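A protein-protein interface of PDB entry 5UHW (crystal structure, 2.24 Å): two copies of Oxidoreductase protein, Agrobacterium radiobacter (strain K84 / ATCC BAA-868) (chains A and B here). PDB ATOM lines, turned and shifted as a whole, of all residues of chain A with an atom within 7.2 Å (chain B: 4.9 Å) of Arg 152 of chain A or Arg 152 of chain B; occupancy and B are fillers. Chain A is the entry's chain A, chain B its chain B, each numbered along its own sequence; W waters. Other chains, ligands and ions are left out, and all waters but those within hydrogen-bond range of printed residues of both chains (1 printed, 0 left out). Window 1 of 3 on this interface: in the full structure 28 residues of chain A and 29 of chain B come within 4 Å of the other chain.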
ATOM      1  N   TRP A 150      14.124  17.547  25.411  1.00  0.00           N
ATOM      2  CA  TRP A 150      13.404  17.014  24.253  1.00  0.00           C
ATOM      3  C   TRP A 150      14.359  16.341  23.288  1.00  0.00           C
ATOM      4  O   TRP A 150      15.496  16.810  23.116  1.00  0.00           O
ATOM      5  CB  TRP A 150      12.676  18.147  23.527  1.00  0.00           C
ATOM      6  CG  TRP A 150      11.816  17.723  22.372  1.00  0.00           C
ATOM      7  CD1 TRP A 150      10.506  17.341  22.424  1.00  0.00           C
ATOM      8  CD2 TRP A 150      12.191  17.692  20.981  1.00  0.00           C
ATOM      9  NE1 TRP A 150      10.043  17.049  21.148  1.00  0.00           N
ATOM     10  CE2 TRP A 150      11.054  17.266  20.248  1.00  0.00           C
ATOM     11  CE3 TRP A 150      13.381  17.979  20.282  1.00  0.00           C
ATOM     12  CZ2 TRP A 150      11.072  17.102  18.862  1.00  0.00           C
ATOM     13  CZ3 TRP A 150      13.391  17.839  18.900  1.00  0.00           C
ATOM     14  CH2 TRP A 150      12.242  17.406  18.206  1.00  0.00           C
ATOM     15  N   GLY A 151      13.880  15.279  22.624  1.00  0.00           N
ATOM     16  CA  GLY A 151      14.672  14.590  21.617  1.00  0.00           C
ATOM     17  C   GLY A 151      13.852  14.034  20.475  1.00  0.00           C
ATOM     18  O   GLY A 151      12.647  13.814  20.611  1.00  0.00           O
ATOM     19  N   ARG A 152      14.517  13.833  19.338  1.00  0.00           N
ATOM     20  CA  ARG A 152      13.951  13.100  18.228  1.00  0.00           C
ATOM     21  C   ARG A 152      15.003  12.137  17.710  1.00  0.00           C
ATOM     22  O   ARG A 152      16.138  12.558  17.398  1.00  0.00           O
ATOM     23  CB  ARG A 152      13.543  14.019  17.104  1.00  0.00           C
ATOM     24  CG  ARG A 152      12.821  13.283  15.984  1.00  0.00           C
ATOM     25  CD  ARG A 152      12.915  13.933  14.625  1.00  0.00           C
ATOM     26  NE  ARG A 152      12.188  13.117  13.641  1.00  0.00           N
ATOM     27  CZ  ARG A 152      12.059  13.423  12.344  1.00  0.00           C
ATOM     28  NH1 ARG A 152      12.570  14.543  11.862  1.00  0.00           N
ATOM     29  NH2 ARG A 152      11.400  12.608  11.527  1.00  0.00           N
ATOM     30  N   PHE A 153      14.608  10.866  17.608  1.00  0.00           N
ATOM     31  CA  PHE A 153      15.451   9.800  17.123  1.00  0.00           C
ATOM     32  C   PHE A 153      14.769   9.169  15.896  1.00  0.00           C
ATOM     33  O   PHE A 153      13.751   8.479  16.026  1.00  0.00           O
ATOM     34  CB  PHE A 153      15.668   8.760  18.242  1.00  0.00           C
ATOM     35  CG  PHE A 153      16.212   9.340  19.537  1.00  0.00           C
ATOM     36  CD1 PHE A 153      15.354   9.809  20.528  1.00  0.00           C
ATOM     37  CD2 PHE A 153      17.583   9.405  19.767  1.00  0.00           C
ATOM     38  CE1 PHE A 153      15.847  10.332  21.707  1.00  0.00           C
ATOM     39  CE2 PHE A 153      18.089   9.937  20.946  1.00  0.00           C
ATOM     40  CZ  PHE A 153      17.217  10.403  21.917  1.00  0.00           C
ATOM     41  N   SER A 154      15.352   9.386  14.716  1.00  0.00           N
ATOM     42  CA  SER A 154      14.682   9.105  13.448  1.00  0.00           C
ATOM     43  C   SER A 154      15.488   8.199  12.527  1.00  0.00           C
ATOM     44  O   SER A 154      16.685   8.404  12.325  1.00  0.00           O
ATOM     45  CB  SER A 154      14.400  10.432  12.738  1.00  0.00           C
ATOM     46  OG  SER A 154      13.435  10.331  11.704  1.00  0.00           O
ATOM     47  N   PHE A 155      14.818   7.194  11.966  1.00  0.00           N
ATOM     48  CA  PHE A 155      15.408   6.294  10.971  1.00  0.00           C
ATOM     49  C   PHE A 155      14.289   6.105   9.984  1.00  0.00           C
ATOM     50  O   PHE A 155      13.358   5.345  10.230  1.00  0.00           O
ATOM     51  CB  PHE A 155      15.855   4.974  11.634  1.00  0.00           C
ATOM     52  CG  PHE A 155      16.610   4.015  10.725  1.00  0.00           C
ATOM     53  CD1 PHE A 155      15.969   3.318   9.706  1.00  0.00           C
ATOM     54  CD2 PHE A 155      17.977   3.769  10.926  1.00  0.00           C
ATOM     55  CE1 PHE A 155      16.659   2.401   8.903  1.00  0.00           C
ATOM     56  CE2 PHE A 155      18.667   2.869  10.128  1.00  0.00           C
ATOM     57  CZ  PHE A 155      18.009   2.184   9.114  1.00  0.00           C
ATOM     58  N   ARG A 156      14.340   6.849   8.899  1.00  0.00           N
ATOM     59  CA  ARG A 156      13.344   6.776   7.826  1.00  0.00           C
ATOM     60  C   ARG A 156      14.110   6.427   6.558  1.00  0.00           C
ATOM     61  O   ARG A 156      14.996   7.165   6.141  1.00  0.00           O
ATOM     62  CB  ARG A 156      12.575   8.105   7.676  1.00  0.00           C
ATOM     63  CG  ARG A 156      12.053   8.687   8.987  1.00  0.00           C
ATOM     64  CD  ARG A 156      11.022   9.791   8.763  1.00  0.00           C
ATOM     65  NE  ARG A 156       9.722   9.270   8.300  1.00  0.00           N
ATOM     66  CZ  ARG A 156       8.832   8.622   9.070  1.00  0.00           C
ATOM     67  NH1 ARG A 156       9.068   8.365  10.366  1.00  0.00           N
ATOM     68  NH2 ARG A 156       7.696   8.192   8.528  1.00  0.00           N
ATOM     69  N   THR A 183      16.417   1.936  17.785  1.00  0.00           N
ATOM     70  CA  THR A 183      16.136   3.373  17.942  1.00  0.00           C
ATOM     71  C   THR A 183      15.658   3.686  19.377  1.00  0.00           C
ATOM     72  O   THR A 183      16.024   4.724  19.968  1.00  0.00           O
ATOM     73  CB  THR A 183      15.120   3.872  16.904  1.00  0.00           C
ATOM     74  OG1 THR A 183      15.317   3.170  15.678  1.00  0.00           O
ATOM     75  CG2 THR A 183      15.299   5.345  16.647  1.00  0.00           C
ATOM     76  N   LEU A 191      18.798   9.643  26.579  1.00  0.00           N
ATOM     77  CA  LEU A 191      17.881  10.402  27.438  1.00  0.00           C
ATOM     78  C   LEU A 191      17.452   9.680  28.711  1.00  0.00           C
ATOM     79  O   LEU A 191      16.721  10.260  29.535  1.00  0.00           O
ATOM     80  CB  LEU A 191      16.655  10.843  26.623  1.00  0.00           C
ATOM     81  CG  LEU A 191      16.900  11.951  25.584  1.00  0.00           C
ATOM     82  CD1 LEU A 191      15.575  12.363  24.964  1.00  0.00           C
ATOM     83  CD2 LEU A 191      17.609  13.180  26.153  1.00  0.00           C
ATOM     84  N   THR A 225      10.985  14.596  27.041  1.00  0.00           N
ATOM     85  CA  THR A 225      10.061  13.995  26.075  1.00  0.00           C
ATOM     86  C   THR A 225      10.831  13.628  24.804  1.00  0.00           C
ATOM     87  O   THR A 225      11.657  14.398  24.360  1.00  0.00           O
ATOM     88  CB  THR A 225       8.952  14.990  25.716  1.00  0.00           C
ATOM     89  OG1 THR A 225       8.350  15.478  26.917  1.00  0.00           O
ATOM     90  CG2 THR A 225       7.880  14.339  24.850  1.00  0.00           C
ATOM     91  N   SER A 226      10.582  12.462  24.226  1.00  0.00           N
ATOM     92  CA  SER A 226      11.135  12.175  22.890  1.00  0.00           C
ATOM     93  C   SER A 226      10.171  11.514  21.862  1.00  0.00           C
ATOM     94  O   SER A 226       9.150  10.887  22.204  1.00  0.00           O
ATOM     95  CB  SER A 226      12.448  11.394  23.012  1.00  0.00           C
ATOM     96  OG  SER A 226      12.189  10.022  23.120  1.00  0.00           O
ATOM     97  N   ILE A 227      10.509  11.715  20.593  1.00  0.00           N
ATOM     98  CA  ILE A 227       9.873  11.041  19.472  1.00  0.00           C
ATOM     99  C   ILE A 227      10.876  10.031  18.934  1.00  0.00           C
ATOM    100  O   ILE A 227      11.998  10.398  18.604  1.00  0.00           O
ATOM    101  CB  ILE A 227       9.557  12.040  18.339  1.00  0.00           C
ATOM    102  CG1 ILE A 227       8.589  13.122  18.817  1.00  0.00           C
ATOM    103  CG2 ILE A 227       9.019  11.353  17.081  1.00  0.00           C
ATOM    104  CD1 ILE A 227       7.219  12.603  19.173  1.00  0.00           C
ATOM    105  N   VAL A 228      10.464   8.777  18.840  1.00  0.00           N
ATOM    106  CA  VAL A 228      11.145   7.768  18.042  1.00  0.00           C
ATOM    107  C   VAL A 228      10.246   7.482  16.836  1.00  0.00           C
ATOM    108  O   VAL A 228       9.110   7.059  17.004  1.00  0.00           O
ATOM    109  CB  VAL A 228      11.384   6.497  18.866  1.00  0.00           C
ATOM    110  CG1 VAL A 228      11.866   5.357  18.005  1.00  0.00           C
ATOM    111  CG2 VAL A 228      12.387   6.780  19.963  1.00  0.00           C
ATOM    112  N   ASP A 229      10.728   7.735  15.631  1.00  0.00           N
ATOM    113  CA  ASP A 229       9.931   7.549  14.451  1.00  0.00           C
ATOM    114  C   ASP A 229      10.739   6.762  13.436  1.00  0.00           C
ATOM    115  O   ASP A 229      11.822   7.166  13.068  1.00  0.00           O
ATOM    116  CB  ASP A 229       9.458   8.905  13.913  1.00  0.00           C
ATOM    117  CG  ASP A 229      10.591   9.785  13.389  1.00  0.00           C
ATOM    118  OD1 ASP A 229      11.234  10.513  14.158  1.00  0.00           O
ATOM    119  OD2 ASP A 229      10.818   9.794  12.168  1.00  0.00           O
ATOM    120  N   THR A 244      20.889   6.888  11.744  1.00  0.00           N
ATOM    121  CA  THR A 244      19.875   7.268  12.690  1.00  0.00           C
ATOM    122  C   THR A 244      20.123   8.748  12.966  1.00  0.00           C
ATOM    123  O   THR A 244      21.180   9.111  13.486  1.00  0.00           O
ATOM    124  CB  THR A 244      20.000   6.439  13.982  1.00  0.00           C
ATOM    125  OG1 THR A 244      19.811   5.036  13.708  1.00  0.00           O
ATOM    126  CG2 THR A 244      18.963   6.908  15.017  1.00  0.00           C
ATOM    127  N   LEU A 245      19.177   9.600  12.597  1.00  0.00           N
ATOM    128  CA  LEU A 245      19.321  11.042  12.771  1.00  0.00           C
ATOM    129  C   LEU A 245      18.801  11.478  14.145  1.00  0.00           C
ATOM    130  O   LEU A 245      17.769  11.013  14.582  1.00  0.00           O
ATOM    131  CB  LEU A 245      18.595  11.741  11.622  1.00  0.00           C
ATOM    132  CG  LEU A 245      19.066  11.287  10.215  1.00  0.00           C
ATOM    133  CD1 LEU A 245      18.433  12.090   9.090  1.00  0.00           C
ATOM    134  CD2 LEU A 245      20.595  11.362  10.084  1.00  0.00           C
ATOM    135  N   ILE A 246      19.514  12.345  14.845  1.00  0.00           N
ATOM    136  CA  ILE A 246      19.176  12.660  16.242  1.00  0.00           C
ATOM    137  C   ILE A 246      19.134  14.158  16.462  1.00  0.00           C
ATOM    138  O   ILE A 246      20.029  14.886  16.047  1.00  0.00           O
ATOM    139  CB  ILE A 246      20.171  12.015  17.228  1.00  0.00           C
ATOM    140  CG1 ILE A 246      20.070  10.488  17.115  1.00  0.00           C
ATOM    141  CG2 ILE A 246      19.931  12.474  18.686  1.00  0.00           C
ATOM    142  CD1 ILE A 246      21.139   9.713  17.857  1.00  0.00           C
ATOM    143  N   ASP A 247      18.070  14.609  17.105  1.00  0.00           N
ATOM    144  CA  ASP A 247      17.940  16.006  17.559  1.00  0.00           C
ATOM    145  C   ASP A 247      17.743  15.995  19.065  1.00  0.00           C
ATOM    146  O   ASP A 247      16.903  15.232  19.555  1.00  0.00           O
ATOM    147  CB  ASP A 247      16.708  16.690  16.926  1.00  0.00           C
ATOM    148  CG  ASP A 247      16.766  16.769  15.381  1.00  0.00           C
ATOM    149  OD1 ASP A 247      17.671  16.224  14.722  1.00  0.00           O
ATOM    150  OD2 ASP A 247      15.876  17.404  14.822  1.00  0.00           O
ATOM    151  N   ILE A 248      18.505  16.809  19.804  1.00  0.00           N
ATOM    152  CA  ILE A 248      18.349  16.934  21.268  1.00  0.00           C
ATOM    153  C   ILE A 248      18.306  18.411  21.612  1.00  0.00           C
ATOM    154  O   ILE A 248      19.197  19.156  21.207  1.00  0.00           O
ATOM    155  CB  ILE A 248      19.521  16.292  22.060  1.00  0.00           C
ATOM    156  CG1 ILE A 248      19.793  14.829  21.628  1.00  0.00           C
ATOM    157  CG2 ILE A 248      19.288  16.389  23.579  1.00  0.00           C
ATOM    158  CD1 ILE A 248      18.747  13.817  22.054  1.00  0.00           C
ATOM    159  N   ASP A 249      17.280  18.836  22.350  1.00  0.00           N
ATOM    160  CA  ASP A 249      17.211  20.212  22.856  1.00  0.00           C
ATOM    161  C   ASP A 249      17.492  20.218  24.333  1.00  0.00           C
ATOM    162  O   ASP A 249      16.884  19.461  25.081  1.00  0.00           O
ATOM    163  CB  ASP A 249      15.847  20.858  22.593  1.00  0.00           C
ATOM    164  CG  ASP A 249      15.612  21.165  21.131  1.00  0.00           C
ATOM    165  OD1 ASP A 249      16.514  20.893  20.299  1.00  0.00           O
ATOM    166  OD2 ASP A 249      14.526  21.691  20.806  1.00  0.00           O
ATOM    167  N   ILE A 255      21.723  19.762  20.017  1.00  0.00           N
ATOM    168  CA  ILE A 255      22.509  18.844  19.217  1.00  0.00           C
ATOM    169  C   ILE A 255      21.650  18.441  18.004  1.00  0.00           C
ATOM    170  O   ILE A 255      20.448  18.133  18.148  1.00  0.00           O
ATOM    171  CB  ILE A 255      22.919  17.574  20.007  1.00  0.00           C
ATOM    172  CG1 ILE A 255      23.880  17.912  21.144  1.00  0.00           C
ATOM    173  CG2 ILE A 255      23.555  16.526  19.089  1.00  0.00           C
ATOM    174  CD1 ILE A 255      23.913  16.842  22.236  1.00  0.00           C
ATOM    175  N   ARG A 256      22.289  18.437  16.828  1.00  0.00           N
ATOM    176  CA  ARG A 256      21.674  18.038  15.564  1.00  0.00           C
ATOM    177  C   ARG A 256      22.650  17.125  14.836  1.00  0.00           C
ATOM    178  O   ARG A 256      23.684  17.579  14.317  1.00  0.00           O
ATOM    179  CB  ARG A 256      21.294  19.267  14.728  1.00  0.00           C
ATOM    180  CG  ARG A 256      20.230  20.168  15.382  1.00  0.00           C
ATOM    181  CD  ARG A 256      18.849  19.507  15.418  1.00  0.00           C
ATOM    182  NE  ARG A 256      17.768  20.367  15.937  1.00  0.00           N
ATOM    183  CZ  ARG A 256      17.444  20.515  17.233  1.00  0.00           C
ATOM    184  NH1 ARG A 256      18.119  19.884  18.221  1.00  0.00           N
ATOM    185  NH2 ARG A 256      16.436  21.319  17.559  1.00  0.00           N
ATOM    186  N   LEU A 257      22.372  15.817  14.905  1.00  0.00           N
ATOM    187  CA  LEU A 257      23.095  14.812  14.129  1.00  0.00           C
ATOM    188  C   LEU A 257      22.235  14.577  12.902  1.00  0.00           C
ATOM    189  O   LEU A 257      21.168  14.005  13.022  1.00  0.00           O
ATOM    190  CB  LEU A 257      23.296  13.520  14.921  1.00  0.00           C
ATOM    191  CG  LEU A 257      23.859  12.309  14.170  1.00  0.00           C
ATOM    192  CD1 LEU A 257      25.276  12.582  13.704  1.00  0.00           C
ATOM    193  CD2 LEU A 257      23.837  11.097  15.067  1.00  0.00           C
ATOM    194  N   TRP B 150       2.237   9.829   6.818  1.00  0.00           N
ATOM    195  CA  TRP B 150       2.990  10.300   7.970  1.00  0.00           C
ATOM    196  C   TRP B 150       3.418  11.734   7.772  1.00  0.00           C
ATOM    197  O   TRP B 150       3.743  12.119   6.655  1.00  0.00           O
ATOM    198  CB  TRP B 150       4.220   9.405   8.225  1.00  0.00           C
ATOM    199  CG  TRP B 150       4.957   9.775   9.476  1.00  0.00           C
ATOM    200  CD1 TRP B 150       4.720   9.324  10.709  1.00  0.00           C
ATOM    201  CD2 TRP B 150       6.050  10.698   9.586  1.00  0.00           C
ATOM    202  NE1 TRP B 150       5.589   9.898  11.608  1.00  0.00           N
ATOM    203  CE2 TRP B 150       6.416  10.749  10.935  1.00  0.00           C
ATOM    204  CE3 TRP B 150       6.766  11.462   8.664  1.00  0.00           C
ATOM    205  CZ2 TRP B 150       7.460  11.535  11.397  1.00  0.00           C
ATOM    206  CZ3 TRP B 150       7.803  12.252   9.122  1.00  0.00           C
ATOM    207  CH2 TRP B 150       8.137  12.286  10.479  1.00  0.00           C
ATOM    208  N   GLY B 151       3.438  12.518   8.849  1.00  0.00           N
ATOM    209  CA  GLY B 151       3.927  13.884   8.754  1.00  0.00           C
ATOM    210  C   GLY B 151       4.558  14.425  10.020  1.00  0.00           C
ATOM    211  O   GLY B 151       4.270  13.959  11.121  1.00  0.00           O
ATOM    212  N   ARG B 152       5.444  15.402   9.839  1.00  0.00           N
ATOM    213  CA  ARG B 152       5.920  16.227  10.926  1.00  0.00           C
ATOM    214  C   ARG B 152       5.722  17.696  10.618  1.00  0.00           C
ATOM    215  O   ARG B 152       6.010  18.138   9.506  1.00  0.00           O
ATOM    216  CB  ARG B 152       7.379  15.992  11.141  1.00  0.00           C
ATOM    217  CG  ARG B 152       7.835  16.507  12.490  1.00  0.00           C
ATOM    218  CD  ARG B 152       9.313  16.764  12.478  1.00  0.00           C
ATOM    219  NE  ARG B 152       9.740  17.447  13.703  1.00  0.00           N
ATOM    220  CZ  ARG B 152      11.001  17.764  13.975  1.00  0.00           C
ATOM    221  NH1 ARG B 152      11.960  17.453  13.116  1.00  0.00           N
ATOM    222  NH2 ARG B 152      11.294  18.390  15.110  1.00  0.00           N
ATOM    223  N   PHE B 153       5.236  18.441  11.612  1.00  0.00           N
ATOM    224  CA  PHE B 153       5.040  19.888  11.522  1.00  0.00           C
ATOM    225  C   PHE B 153       5.737  20.499  12.744  1.00  0.00           C
ATOM    226  O   PHE B 153       5.307  20.281  13.864  1.00  0.00           O
ATOM    227  CB  PHE B 153       3.543  20.244  11.488  1.00  0.00           C
ATOM    228  CG  PHE B 153       2.765  19.463  10.462  1.00  0.00           C
ATOM    229  CD1 PHE B 153       2.200  18.231  10.781  1.00  0.00           C
ATOM    230  CD2 PHE B 153       2.642  19.924   9.165  1.00  0.00           C
ATOM    231  CE1 PHE B 153       1.529  17.481   9.827  1.00  0.00           C
ATOM    232  CE2 PHE B 153       1.975  19.176   8.215  1.00  0.00           C
ATOM    233  CZ  PHE B 153       1.420  17.953   8.551  1.00  0.00           C
ATOM    234  N   SER B 154       6.802  21.259  12.505  1.00  0.00           N
ATOM    235  CA  SER B 154       7.748  21.625  13.540  1.00  0.00           C
ATOM    236  C   SER B 154       8.021  23.131  13.525  1.00  0.00           C
ATOM    237  O   SER B 154       8.286  23.727  12.469  1.00  0.00           O
ATOM    238  CB  SER B 154       9.049  20.871  13.309  1.00  0.00           C
ATOM    239  OG  SER B 154       9.958  21.061  14.363  1.00  0.00           O
ATOM    240  N   ARG B 156      10.455  25.334  16.055  1.00  0.00           N
ATOM    241  CA  ARG B 156      11.384  25.322  17.177  1.00  0.00           C
ATOM    242  C   ARG B 156      12.250  26.580  17.071  1.00  0.00           C
ATOM    243  O   ARG B 156      13.002  26.742  16.114  1.00  0.00           O
ATOM    244  CB  ARG B 156      12.262  24.055  17.149  1.00  0.00           C
ATOM    245  CG  ARG B 156      11.472  22.760  17.122  1.00  0.00           C
ATOM    246  CD  ARG B 156      12.293  21.547  17.537  1.00  0.00           C
ATOM    247  NE  ARG B 156      12.430  21.408  18.990  1.00  0.00           N
ATOM    248  CZ  ARG B 156      11.473  21.004  19.832  1.00  0.00           C
ATOM    249  NH1 ARG B 156      10.247  20.682  19.407  1.00  0.00           N
ATOM    250  NH2 ARG B 156      11.735  20.931  21.129  1.00  0.00           N
ATOM    251  N   SER B 226       0.740  12.001  12.494  1.00  0.00           N
ATOM    252  CA  SER B 226       1.687  13.126  12.471  1.00  0.00           C
ATOM    253  C   SER B 226       2.160  13.624  13.835  1.00  0.00           C
ATOM    254  O   SER B 226       1.593  13.316  14.875  1.00  0.00           O
ATOM    255  CB  SER B 226       1.135  14.290  11.690  1.00  0.00           C
ATOM    256  OG  SER B 226       0.204  15.003  12.443  1.00  0.00           O
ATOM    257  N   ILE B 227       3.245  14.373  13.789  1.00  0.00           N
ATOM    258  CA  ILE B 227       3.862  14.937  14.940  1.00  0.00           C
ATOM    259  C   ILE B 227       3.801  16.429  14.766  1.00  0.00           C
ATOM    260  O   ILE B 227       4.217  16.942  13.745  1.00  0.00           O
ATOM    261  CB  ILE B 227       5.323  14.503  15.031  1.00  0.00           C
ATOM    262  CG1 ILE B 227       5.418  12.978  15.207  1.00  0.00           C
ATOM    263  CG2 ILE B 227       6.038  15.190  16.201  1.00  0.00           C
ATOM    264  CD1 ILE B 227       4.839  12.461  16.522  1.00  0.00           C
ATOM    265  N   ASP B 229       5.449  19.333  16.774  1.00  0.00           N
ATOM    266  CA  ASP B 229       6.317  19.744  17.878  1.00  0.00           C
ATOM    267  C   ASP B 229       6.623  21.218  17.784  1.00  0.00           C
ATOM    268  O   ASP B 229       7.036  21.701  16.738  1.00  0.00           O
ATOM    269  CB  ASP B 229       7.600  18.920  17.931  1.00  0.00           C
ATOM    270  CG  ASP B 229       8.408  19.008  16.665  1.00  0.00           C
ATOM    271  OD1 ASP B 229       8.012  18.384  15.657  1.00  0.00           O
ATOM    272  OD2 ASP B 229       9.459  19.693  16.675  1.00  0.00           O
ATOM    273  N   LEU B 245       8.535  24.046   9.584  1.00  0.00           N
ATOM    274  CA  LEU B 245       9.201  23.012   8.774  1.00  0.00           C
ATOM    275  C   LEU B 245       8.336  21.780   8.681  1.00  0.00           C
ATOM    276  O   LEU B 245       7.788  21.353   9.667  1.00  0.00           O
ATOM    277  CB  LEU B 245      10.556  22.669   9.392  1.00  0.00           C
ATOM    278  CG  LEU B 245      11.383  23.923   9.745  1.00  0.00           C
ATOM    279  CD1 LEU B 245      12.764  23.533  10.220  1.00  0.00           C
ATOM    280  CD2 LEU B 245      11.444  24.925   8.588  1.00  0.00           C
ATOM    281  N   ILE B 246       8.222  21.208   7.497  1.00  0.00           N
ATOM    282  CA  ILE B 246       7.239  20.176   7.246  1.00  0.00           C
ATOM    283  C   ILE B 246       7.845  18.982   6.531  1.00  0.00           C
ATOM    284  O   ILE B 246       8.541  19.121   5.556  1.00  0.00           O
ATOM    285  CB  ILE B 246       6.072  20.735   6.395  1.00  0.00           C
ATOM    286  CG1 ILE B 246       5.525  21.989   7.078  1.00  0.00           C
ATOM    287  CG2 ILE B 246       4.985  19.672   6.186  1.00  0.00           C
ATOM    288  CD1 ILE B 246       4.238  22.547   6.507  1.00  0.00           C
ATOM    289  N   ASP B 247       7.533  17.798   7.020  1.00  0.00           N
ATOM    290  CA  ASP B 247       7.887  16.569   6.330  1.00  0.00           C
ATOM    291  C   ASP B 247       6.613  15.777   6.112  1.00  0.00           C
ATOM    292  O   ASP B 247       5.836  15.613   7.040  1.00  0.00           O
ATOM    293  CB  ASP B 247       8.855  15.727   7.159  1.00  0.00           C
ATOM    294  CG  ASP B 247      10.095  16.501   7.593  1.00  0.00           C
ATOM    295  OD1 ASP B 247      10.364  17.633   7.154  1.00  0.00           O
ATOM    296  OD2 ASP B 247      10.832  15.949   8.399  1.00  0.00           O
HETATM  297  O   HOH W   1       7.035   7.041  11.742  1.00  0.00           O
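OD2 of Asp 249 of chain A is in salt-bridge range of NE of Arg 156 of chain B, 2.8 Å away.
The guanidinium group of Arg 152 of chain A sits close to the guanidinium group of Arg 152 of chain B, at 3.2 Å.
The guanidinium group of Arg 152 of chain A lies within hydrogen-bond range of the side-chain hydroxyl of Ser 154 of chain A.
The backbone NH (N) of Ile 227 of chain A is in hydrogen-bond range of the backbone carbonyl oxygen (O) of Gly 151 of chain A (3.0 Å).
The side-chain carboxylate of Asp 249 of chain A is in salt-bridge range of the guanidinium group of Arg 256 of chain A (2.8 Å).
The backbone carbonyl oxygen (O) of Phe 153 of chain A sits at hydrogen-bond distance from the backbone NH (N) of Asp 229 of chain A (3.1 Å).
The backbone NH of Phe 153 of chain B lies within hydrogen-bond range of the backbone carbonyl oxygen of Ile 227 of chain B (2.8 Å).
NH1 of Arg 156 of chain A lies within salt-bridge range of OD2 of Asp 229 of chain A (2.9 Å).
Among the printed residues, merely in contact across the chains: Trp 150 of chain A with Arg 152 of chain B (3.4 Å), Trp 150 of chain A with Arg 156 of chain B (3.3 Å), Trp 150 of chain A with Asp 229 of chain B (3.8 Å), Arg 152 of chain A with Trp 150 of chain B (3.4 Å), Arg 156 of chain A with Trp 150 of chain B (3.2 Å), Ile 227 of chain A with Ile 227 of chain B (3.6 Å) and Asp 229 of chain A with Trp 150 of chain B (3.9 Å).
Of the printed residues of chain B, Arg 152 of chain A touches Trp 150 and Arg 152.
Printed residues of chain A within 4 Å of Arg 152 of chain B: Trp 150 (3.4 Å) and Arg 152 (3.2 Å).
Printed residues of chain B within 4 Å of Arg 156 of chain A: Trp 150.
Of the printed residues of chain A, Trp 150 of chain B touches Arg 152, Arg 156 and Asp 229.
Of the printed residues of chain B, Asp 229 of chain A touches Trp 150 (3.9 Å).
Ile 246 of chain A touches none of the printed residues of chain B.
The nearest printed residue of chain A that does not touch Arg 156 of chain B is Arg 256 of chain A (4.1 Å).
Of the 23 printed residues of chain A, 6 touch a printed residue of chain B.
Hydrophobic or aromatic side chains of chain A within 4 Å of the printed part of chain B: Trp 150 and Ile 227.
Among the printed residues, 9 pairs touch across the chains.
Trp 150 of chain A touches Arg 156 of chain B, and with the chains exchanged Arg 156 of chain A touches Trp 150 of chain B.
Trp 150 of chain A touches Asp 229 of chain B, and with the chains exchanged Asp 229 of chain A touches Trp 150 of chain B.
Arg 152 of chain B touches its own counterpart, Arg 152 of chain A.
Ile 227 of chain B touches its own counterpart, Ile 227 of chain A.
12 positions are printed for both chains.
Of the 9 pairs that touch across the chains among the printed residues, 8 have their exchanged pair printed and touching as well.
Water W1 bridges the guanidinium group of Arg 156 of chain A and the indole nitrogen of Trp 150 of chain B.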
